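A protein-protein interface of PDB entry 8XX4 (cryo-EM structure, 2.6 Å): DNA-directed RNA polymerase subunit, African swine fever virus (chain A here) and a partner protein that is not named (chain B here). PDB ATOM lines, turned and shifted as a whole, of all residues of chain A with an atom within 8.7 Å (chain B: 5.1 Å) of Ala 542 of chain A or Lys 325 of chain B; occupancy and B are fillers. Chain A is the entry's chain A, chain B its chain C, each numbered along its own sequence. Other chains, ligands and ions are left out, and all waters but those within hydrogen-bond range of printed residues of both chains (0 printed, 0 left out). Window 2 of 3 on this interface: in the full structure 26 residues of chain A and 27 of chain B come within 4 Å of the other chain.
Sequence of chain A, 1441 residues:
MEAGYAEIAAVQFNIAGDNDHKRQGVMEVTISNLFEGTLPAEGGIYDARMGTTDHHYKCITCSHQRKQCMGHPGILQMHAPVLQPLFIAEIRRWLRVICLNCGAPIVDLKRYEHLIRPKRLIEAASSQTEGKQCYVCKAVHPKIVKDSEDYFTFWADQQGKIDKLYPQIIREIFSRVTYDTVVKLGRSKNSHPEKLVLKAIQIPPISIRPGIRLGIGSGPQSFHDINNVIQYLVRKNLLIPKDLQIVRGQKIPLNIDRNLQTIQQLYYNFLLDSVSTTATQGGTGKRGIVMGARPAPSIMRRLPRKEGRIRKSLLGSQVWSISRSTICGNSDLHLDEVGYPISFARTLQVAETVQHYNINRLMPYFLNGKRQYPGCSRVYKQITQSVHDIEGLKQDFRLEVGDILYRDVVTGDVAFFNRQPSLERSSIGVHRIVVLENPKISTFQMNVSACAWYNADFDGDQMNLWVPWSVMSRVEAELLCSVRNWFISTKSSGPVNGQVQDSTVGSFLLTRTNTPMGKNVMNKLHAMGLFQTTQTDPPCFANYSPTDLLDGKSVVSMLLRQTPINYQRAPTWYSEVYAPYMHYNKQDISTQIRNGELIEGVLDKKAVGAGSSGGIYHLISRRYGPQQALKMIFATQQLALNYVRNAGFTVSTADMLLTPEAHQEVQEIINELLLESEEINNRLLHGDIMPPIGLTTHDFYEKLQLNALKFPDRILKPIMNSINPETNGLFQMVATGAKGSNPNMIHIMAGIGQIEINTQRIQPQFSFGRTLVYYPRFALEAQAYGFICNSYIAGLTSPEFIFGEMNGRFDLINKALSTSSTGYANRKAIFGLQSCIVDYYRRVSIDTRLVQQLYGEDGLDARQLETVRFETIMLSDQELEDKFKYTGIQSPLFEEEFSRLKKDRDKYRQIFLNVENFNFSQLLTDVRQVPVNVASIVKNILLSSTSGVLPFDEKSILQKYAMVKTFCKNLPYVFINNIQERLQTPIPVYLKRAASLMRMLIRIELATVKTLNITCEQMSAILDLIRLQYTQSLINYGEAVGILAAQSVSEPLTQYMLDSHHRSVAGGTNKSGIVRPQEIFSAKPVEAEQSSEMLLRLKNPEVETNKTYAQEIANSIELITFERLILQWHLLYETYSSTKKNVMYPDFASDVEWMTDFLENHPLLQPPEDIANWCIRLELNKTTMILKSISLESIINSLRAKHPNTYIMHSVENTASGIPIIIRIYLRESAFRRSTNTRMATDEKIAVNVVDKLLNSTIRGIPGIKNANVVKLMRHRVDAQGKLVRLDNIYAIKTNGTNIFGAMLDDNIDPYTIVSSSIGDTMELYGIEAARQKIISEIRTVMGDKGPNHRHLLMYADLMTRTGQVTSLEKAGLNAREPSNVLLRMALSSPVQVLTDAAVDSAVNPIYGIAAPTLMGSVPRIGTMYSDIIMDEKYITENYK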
ATOM      1  N   LYS A 524      21.532  -7.844  12.831  1.00  0.00           N
ATOM      2  CA  LYS A 524      20.187  -8.395  12.707  1.00  0.00           C
ATOM      3  C   LYS A 524      19.537  -8.594  14.069  1.00  0.00           C
ATOM      4  O   LYS A 524      18.324  -8.412  14.215  1.00  0.00           O
ATOM      5  CB  LYS A 524      20.230  -9.709  11.934  1.00  0.00           C
ATOM      6  CG  LYS A 524      18.894 -10.411  11.822  1.00  0.00           C
ATOM      7  CD  LYS A 524      19.089 -11.894  11.634  1.00  0.00           C
ATOM      8  CE  LYS A 524      17.772 -12.619  11.569  1.00  0.00           C
ATOM      9  NZ  LYS A 524      17.829 -13.754  10.623  1.00  0.00           N
ATOM     10  N   MET A 528      16.069  -6.842  15.127  1.00  0.00           N
ATOM     11  CA  MET A 528      14.955  -7.629  15.645  1.00  0.00           C
ATOM     12  C   MET A 528      14.501  -7.115  17.004  1.00  0.00           C
ATOM     13  O   MET A 528      13.300  -6.972  17.252  1.00  0.00           O
ATOM     14  CB  MET A 528      15.352  -9.101  15.743  1.00  0.00           C
ATOM     15  CG  MET A 528      15.031  -9.919  14.517  1.00  0.00           C
ATOM     16  SD  MET A 528      15.526 -11.644  14.622  1.00  0.00           S
ATOM     17  CE  MET A 528      17.007 -11.517  15.609  1.00  0.00           C
ATOM     18  N   PRO A 539       8.203  -7.902  11.728  1.00  0.00           N
ATOM     19  CA  PRO A 539       8.588  -8.128  10.330  1.00  0.00           C
ATOM     20  C   PRO A 539       9.425  -9.384  10.161  1.00  0.00           C
ATOM     21  O   PRO A 539       9.636 -10.134  11.117  1.00  0.00           O
ATOM     22  CB  PRO A 539       9.381  -6.864   9.978  1.00  0.00           C
ATOM     23  CG  PRO A 539       9.825  -6.322  11.273  1.00  0.00           C
ATOM     24  CD  PRO A 539       8.772  -6.659  12.264  1.00  0.00           C
ATOM     25  N   CYS A 540       9.894  -9.632   8.945  1.00  0.00           N
ATOM     26  CA  CYS A 540      10.678 -10.817   8.636  1.00  0.00           C
ATOM     27  C   CYS A 540      12.138 -10.427   8.463  1.00  0.00           C
ATOM     28  O   CYS A 540      12.453  -9.489   7.724  1.00  0.00           O
ATOM     29  CB  CYS A 540      10.157 -11.501   7.373  1.00  0.00           C
ATOM     30  SG  CYS A 540      10.962 -13.062   6.967  1.00  0.00           S
ATOM     31  N   PHE A 541      13.022 -11.141   9.155  1.00  0.00           N
ATOM     32  CA  PHE A 541      14.458 -10.938   9.046  1.00  0.00           C
ATOM     33  C   PHE A 541      15.160 -12.164   8.482  1.00  0.00           C
ATOM     34  O   PHE A 541      16.378 -12.298   8.627  1.00  0.00           O
ATOM     35  CB  PHE A 541      15.051 -10.578  10.407  1.00  0.00           C
ATOM     36  CG  PHE A 541      14.536  -9.295  10.975  1.00  0.00           C
ATOM     37  CD1 PHE A 541      13.346  -9.263  11.674  1.00  0.00           C
ATOM     38  CD2 PHE A 541      15.245  -8.123  10.823  1.00  0.00           C
ATOM     39  CE1 PHE A 541      12.874  -8.091  12.205  1.00  0.00           C
ATOM     40  CE2 PHE A 541      14.772  -6.950  11.349  1.00  0.00           C
ATOM     41  CZ  PHE A 541      13.587  -6.936  12.044  1.00  0.00           C
ATOM     42  N   ALA A 542      14.413 -13.069   7.848  1.00  0.00           N
ATOM     43  CA  ALA A 542      15.007 -14.305   7.355  1.00  0.00           C
ATOM     44  C   ALA A 542      16.041 -14.044   6.271  1.00  0.00           C
ATOM     45  O   ALA A 542      16.979 -14.830   6.111  1.00  0.00           O
ATOM     46  CB  ALA A 542      13.918 -15.239   6.837  1.00  0.00           C
ATOM     47  N   ASN A 543      15.897 -12.951   5.527  1.00  0.00           N
ATOM     48  CA  ASN A 543      16.848 -12.612   4.480  1.00  0.00           C
ATOM     49  C   ASN A 543      18.073 -11.880   5.007  1.00  0.00           C
ATOM     50  O   ASN A 543      18.957 -11.541   4.216  1.00  0.00           O
ATOM     51  CB  ASN A 543      16.166 -11.767   3.401  1.00  0.00           C
ATOM     52  CG  ASN A 543      15.291 -10.677   3.981  1.00  0.00           C
ATOM     53  OD1 ASN A 543      14.840 -10.768   5.122  1.00  0.00           O
ATOM     54  ND2 ASN A 543      15.039  -9.639   3.193  1.00  0.00           N
ATOM     55  N   TYR A 544      18.148 -11.628   6.309  1.00  0.00           N
ATOM     56  CA  TYR A 544      19.267 -10.922   6.916  1.00  0.00           C
ATOM     57  C   TYR A 544      20.127 -11.903   7.697  1.00  0.00           C
ATOM     58  O   TYR A 544      19.618 -12.652   8.534  1.00  0.00           O
ATOM     59  CB  TYR A 544      18.775  -9.810   7.840  1.00  0.00           C
ATOM     60  CG  TYR A 544      18.081  -8.683   7.124  1.00  0.00           C
ATOM     61  CD1 TYR A 544      18.794  -7.785   6.353  1.00  0.00           C
ATOM     62  CD2 TYR A 544      16.711  -8.515   7.223  1.00  0.00           C
ATOM     63  CE1 TYR A 544      18.166  -6.754   5.697  1.00  0.00           C
ATOM     64  CE2 TYR A 544      16.073  -7.489   6.572  1.00  0.00           C
ATOM     65  CZ  TYR A 544      16.805  -6.610   5.810  1.00  0.00           C
ATOM     66  OH  TYR A 544      16.172  -5.579   5.158  1.00  0.00           O
ATOM     67  N   SER A 545      21.422 -11.900   7.415  1.00  0.00           N
ATOM     68  CA  SER A 545      22.370 -12.713   8.151  1.00  0.00           C
ATOM     69  C   SER A 545      22.790 -11.993   9.429  1.00  0.00           C
ATOM     70  O   SER A 545      22.663 -10.773   9.531  1.00  0.00           O
ATOM     71  CB  SER A 545      23.581 -13.014   7.275  1.00  0.00           C
ATOM     72  OG  SER A 545      24.730 -13.310   8.046  1.00  0.00           O
ATOM     73  N   PRO A 546      23.272 -12.731  10.432  1.00  0.00           N
ATOM     74  CA  PRO A 546      23.737 -12.066  11.660  1.00  0.00           C
ATOM     75  C   PRO A 546      24.808 -11.026  11.414  1.00  0.00           C
ATOM     76  O   PRO A 546      24.889 -10.042  12.159  1.00  0.00           O
ATOM     77  CB  PRO A 546      24.275 -13.222  12.512  1.00  0.00           C
ATOM     78  CG  PRO A 546      23.658 -14.433  11.981  1.00  0.00           C
ATOM     79  CD  PRO A 546      23.115 -14.182  10.610  1.00  0.00           C
ATOM     80  N   ASP A 548      24.929  -9.091   8.796  1.00  0.00           N
ATOM     81  CA  ASP A 548      24.391  -7.979   8.026  1.00  0.00           C
ATOM     82  C   ASP A 548      24.129  -6.777   8.922  1.00  0.00           C
ATOM     83  O   ASP A 548      23.801  -6.921  10.101  1.00  0.00           O
ATOM     84  CB  ASP A 548      23.101  -8.396   7.324  1.00  0.00           C
ATOM     85  CG  ASP A 548      23.353  -9.217   6.078  1.00  0.00           C
ATOM     86  OD1 ASP A 548      24.528  -9.516   5.789  1.00  0.00           O
ATOM     87  OD2 ASP A 548      22.375  -9.565   5.388  1.00  0.00           O
ATOM     88  N   GLU B 273       3.776 -18.698   4.901  1.00  0.00           N
ATOM     89  CA  GLU B 273       4.739 -19.281   3.980  1.00  0.00           C
ATOM     90  C   GLU B 273       5.647 -20.271   4.692  1.00  0.00           C
ATOM     91  O   GLU B 273       6.843 -20.011   4.856  1.00  0.00           O
ATOM     92  CB  GLU B 273       5.568 -18.178   3.320  1.00  0.00           C
ATOM     93  CG  GLU B 273       4.743 -16.994   2.841  1.00  0.00           C
ATOM     94  CD  GLU B 273       5.448 -15.668   3.048  1.00  0.00           C
ATOM     95  OE1 GLU B 273       6.490 -15.648   3.735  1.00  0.00           O
ATOM     96  OE2 GLU B 273       4.959 -14.644   2.525  1.00  0.00           O
ATOM     97  N   GLU B 274       5.073 -21.390   5.148  1.00  0.00           N
ATOM     98  CA  GLU B 274       5.792 -22.441   5.862  1.00  0.00           C
ATOM     99  C   GLU B 274       6.240 -21.931   7.230  1.00  0.00           C
ATOM    100  O   GLU B 274       6.741 -22.696   8.058  1.00  0.00           O
ATOM    101  CB  GLU B 274       6.967 -22.953   5.006  1.00  0.00           C
ATOM    102  CG  GLU B 274       8.018 -23.824   5.699  1.00  0.00           C
ATOM    103  CD  GLU B 274       7.560 -25.249   5.950  1.00  0.00           C
ATOM    104  OE1 GLU B 274       6.358 -25.543   5.776  1.00  0.00           O
ATOM    105  OE2 GLU B 274       8.412 -26.081   6.322  1.00  0.00           O
ATOM    106  N   LYS B 275       5.999 -20.653   7.505  1.00  0.00           N
ATOM    107  CA  LYS B 275       6.410 -20.071   8.772  1.00  0.00           C
ATOM    108  C   LYS B 275       5.451 -20.468   9.884  1.00  0.00           C
ATOM    109  O   LYS B 275       4.231 -20.459   9.708  1.00  0.00           O
ATOM    110  CB  LYS B 275       6.486 -18.549   8.657  1.00  0.00           C
ATOM    111  CG  LYS B 275       7.884 -18.038   8.341  1.00  0.00           C
ATOM    112  CD  LYS B 275       7.963 -16.523   8.276  1.00  0.00           C
ATOM    113  CE  LYS B 275       6.795 -15.920   7.521  1.00  0.00           C
ATOM    114  NZ  LYS B 275       6.653 -14.465   7.805  1.00  0.00           N
ATOM    115  N   ASP B 303      19.444 -17.634  10.512  1.00  0.00           N
ATOM    116  CA  ASP B 303      18.521 -17.154   9.494  1.00  0.00           C
ATOM    117  C   ASP B 303      17.074 -17.106   9.980  1.00  0.00           C
ATOM    118  O   ASP B 303      16.151 -17.101   9.159  1.00  0.00           O
ATOM    119  CB  ASP B 303      18.690 -17.985   8.213  1.00  0.00           C
ATOM    120  CG  ASP B 303      17.992 -19.358   8.249  1.00  0.00           C
ATOM    121  OD1 ASP B 303      17.003 -19.589   8.975  1.00  0.00           O
ATOM    122  OD2 ASP B 303      18.467 -20.247   7.514  1.00  0.00           O
ATOM    123  N   ILE B 304      16.866 -17.044  11.296  1.00  0.00           N
ATOM    124  CA  ILE B 304      15.519 -17.013  11.851  1.00  0.00           C
ATOM    125  C   ILE B 304      14.767 -15.796  11.333  1.00  0.00           C
ATOM    126  O   ILE B 304      15.342 -14.723  11.127  1.00  0.00           O
ATOM    127  CB  ILE B 304      15.584 -17.021  13.388  1.00  0.00           C
ATOM    128  CG1 ILE B 304      14.199 -17.239  13.990  1.00  0.00           C
ATOM    129  CG2 ILE B 304      16.205 -15.742  13.914  1.00  0.00           C
ATOM    130  CD1 ILE B 304      14.224 -18.039  15.246  1.00  0.00           C
ATOM    131  N   SER B 305      13.468 -15.972  11.090  1.00  0.00           N
ATOM    132  CA  SER B 305      12.650 -14.854  10.638  1.00  0.00           C
ATOM    133  C   SER B 305      12.541 -13.788  11.717  1.00  0.00           C
ATOM    134  O   SER B 305      12.747 -12.600  11.453  1.00  0.00           O
ATOM    135  CB  SER B 305      11.268 -15.352  10.221  1.00  0.00           C
ATOM    136  OG  SER B 305      10.409 -14.273   9.913  1.00  0.00           O
ATOM    137  N   ILE B 323       9.492 -16.827  15.227  1.00  0.00           N
ATOM    138  CA  ILE B 323       8.917 -17.044  13.908  1.00  0.00           C
ATOM    139  C   ILE B 323      10.009 -17.614  13.022  1.00  0.00           C
ATOM    140  O   ILE B 323      11.098 -17.040  12.928  1.00  0.00           O
ATOM    141  CB  ILE B 323       8.350 -15.745  13.311  1.00  0.00           C
ATOM    142  CG1 ILE B 323       7.447 -15.050  14.326  1.00  0.00           C
ATOM    143  CG2 ILE B 323       7.603 -16.036  12.025  1.00  0.00           C
ATOM    144  CD1 ILE B 323       6.547 -14.013  13.725  1.00  0.00           C
ATOM    145  N   HIS B 324       9.728 -18.745  12.382  1.00  0.00           N
ATOM    146  CA  HIS B 324      10.749 -19.432  11.610  1.00  0.00           C
ATOM    147  C   HIS B 324      10.117 -20.122  10.414  1.00  0.00           C
ATOM    148  O   HIS B 324       8.993 -20.619  10.501  1.00  0.00           O
ATOM    149  CB  HIS B 324      11.493 -20.455  12.470  1.00  0.00           C
ATOM    150  CG  HIS B 324      12.690 -21.048  11.799  1.00  0.00           C
ATOM    151  ND1 HIS B 324      13.429 -20.364  10.859  1.00  0.00           N
ATOM    152  CD2 HIS B 324      13.275 -22.260  11.929  1.00  0.00           C
ATOM    153  CE1 HIS B 324      14.418 -21.129  10.438  1.00  0.00           C
ATOM    154  NE2 HIS B 324      14.347 -22.285  11.071  1.00  0.00           N
ATOM    155  N   LYS B 325      10.854 -20.157   9.303  1.00  0.00           N
ATOM    156  CA  LYS B 325      10.448 -20.899   8.109  1.00  0.00           C
ATOM    157  C   LYS B 325      10.779 -22.371   8.330  1.00  0.00           C
ATOM    158  O   LYS B 325      11.782 -22.899   7.846  1.00  0.00           O
ATOM    159  CB  LYS B 325      11.147 -20.358   6.869  1.00  0.00           C
ATOM    160  CG  LYS B 325      10.561 -19.083   6.300  1.00  0.00           C
ATOM    161  CD  LYS B 325      11.648 -18.232   5.665  1.00  0.00           C
ATOM    162  CE  LYS B 325      11.082 -16.951   5.080  1.00  0.00           C
ATOM    163  NZ  LYS B 325      11.803 -16.540   3.844  1.00  0.00           N
ATOM    164  N   ALA B 326       9.917 -23.040   9.087  1.00  0.00           N
ATOM    165  CA  ALA B 326      10.103 -24.451   9.396  1.00  0.00           C
ATOM    166  C   ALA B 326       8.769 -25.019   9.845  1.00  0.00           C
ATOM    167  O   ALA B 326       7.800 -24.288  10.042  1.00  0.00           O
ATOM    168  CB  ALA B 326      11.177 -24.655  10.467  1.00  0.00           C
ATOM    169  N   SER B 327       8.722 -26.339   9.991  1.00  0.00           N
ATOM    170  CA  SER B 327       7.536 -26.971  10.541  1.00  0.00           C
ATOM    171  C   SER B 327       7.509 -26.798  12.056  1.00  0.00           C
ATOM    172  O   SER B 327       8.494 -26.400  12.681  1.00  0.00           O
ATOM    173  CB  SER B 327       7.495 -28.450  10.172  1.00  0.00           C
ATOM    174  OG  SER B 327       8.471 -29.177  10.893  1.00  0.00           O
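The backbone carbonyl oxygen (O) of Ser 305 of chain B is in hydrogen-bond range of the backbone NH (N) of Phe 541 of chain A (2.7 Å).
SG of Cys 540 of chain A lies within hydrogen-bond range of OG of Ser 305 of chain B.
NZ of Lys 524 of chain A sits at hydrogen-bond distance from O of Ile 304 of chain B, 2.7 Å away.
O of Ile 323 of chain B lies within hydrogen-bond range of N of Ser 305 of chain B (3.2 Å).
The side-chain sulfur (SG) of Cys 540 of chain A lies close to the backbone NH (N) of Ala 542 of chain A.
The backbone carbonyl oxygen (O) of Tyr 544 of chain A lies within hydrogen-bond range of the side-chain amino group (NZ) of Lys 524 of chain A, 3.0 Å away.
The side-chain amino group of Lys 524 of chain A is in hydrogen-bond range of the backbone carbonyl oxygen of Phe 541 of chain A, 2.9 Å away.
Among the printed residues, merely in contact across the chains: Lys 524 of chain A with Asp 303 of chain B (3.5 Å), Ala 542 of chain A with Asp 303 of chain B (3.5 Å), Phe 541 of chain A with Ile 304 of chain B (3.6 Å), Ala 542 of chain A with Lys 325 of chain B (3.7 Å), Ala 542 of chain A with Ser 305 of chain B (3.8 Å), Ala 542 of chain A with Ile 304 of chain B (3.8 Å) and Pro 539 of chain A with Ser 305 of chain B (3.98 Å).
Printed residues of chain B within 4 Å of Pro 539 of chain A: Ser 305 (3.98 Å).
Printed residues of chain B within 4 Å of Cys 540 of chain A: Ser 305 (3.2 Å).
Of the printed residues of chain B, Ala 542 of chain A touches Asp 303 (3.5 Å), Ile 304 (3.8 Å), Ser 305 (3.8 Å) and Lys 325 (3.7 Å).
Printed residues of chain A within 4 Å of Ile 304 of chain B: Lys 524, Phe 541 and Ala 542.
No residue of chain A comes within 4 Å of His 324 of chain B.
Of chain A, only Ala 542 comes within 4 Å of Lys 325 of chain B.
No residue of chain A comes within 4 Å of Ala 326 of chain B.
The nearest printed residue of chain B that does not touch Pro 539 of chain A is Ile 323 of chain B (5.6 Å).
Of the 11 printed residues of chain A, 5 touch a printed residue of chain B.
Hydrophobic or aromatic side chains of chain A within 4 Å of the printed part of chain B: Phe 541 and Ala 542.
Of the 11 printed residues of chain B, 4 touch a printed residue of chain A.
Among the printed residues, no Asp or Glu carboxylate lies within 4 Å of a Lys or Arg side-chain nitrogen of the other chain.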
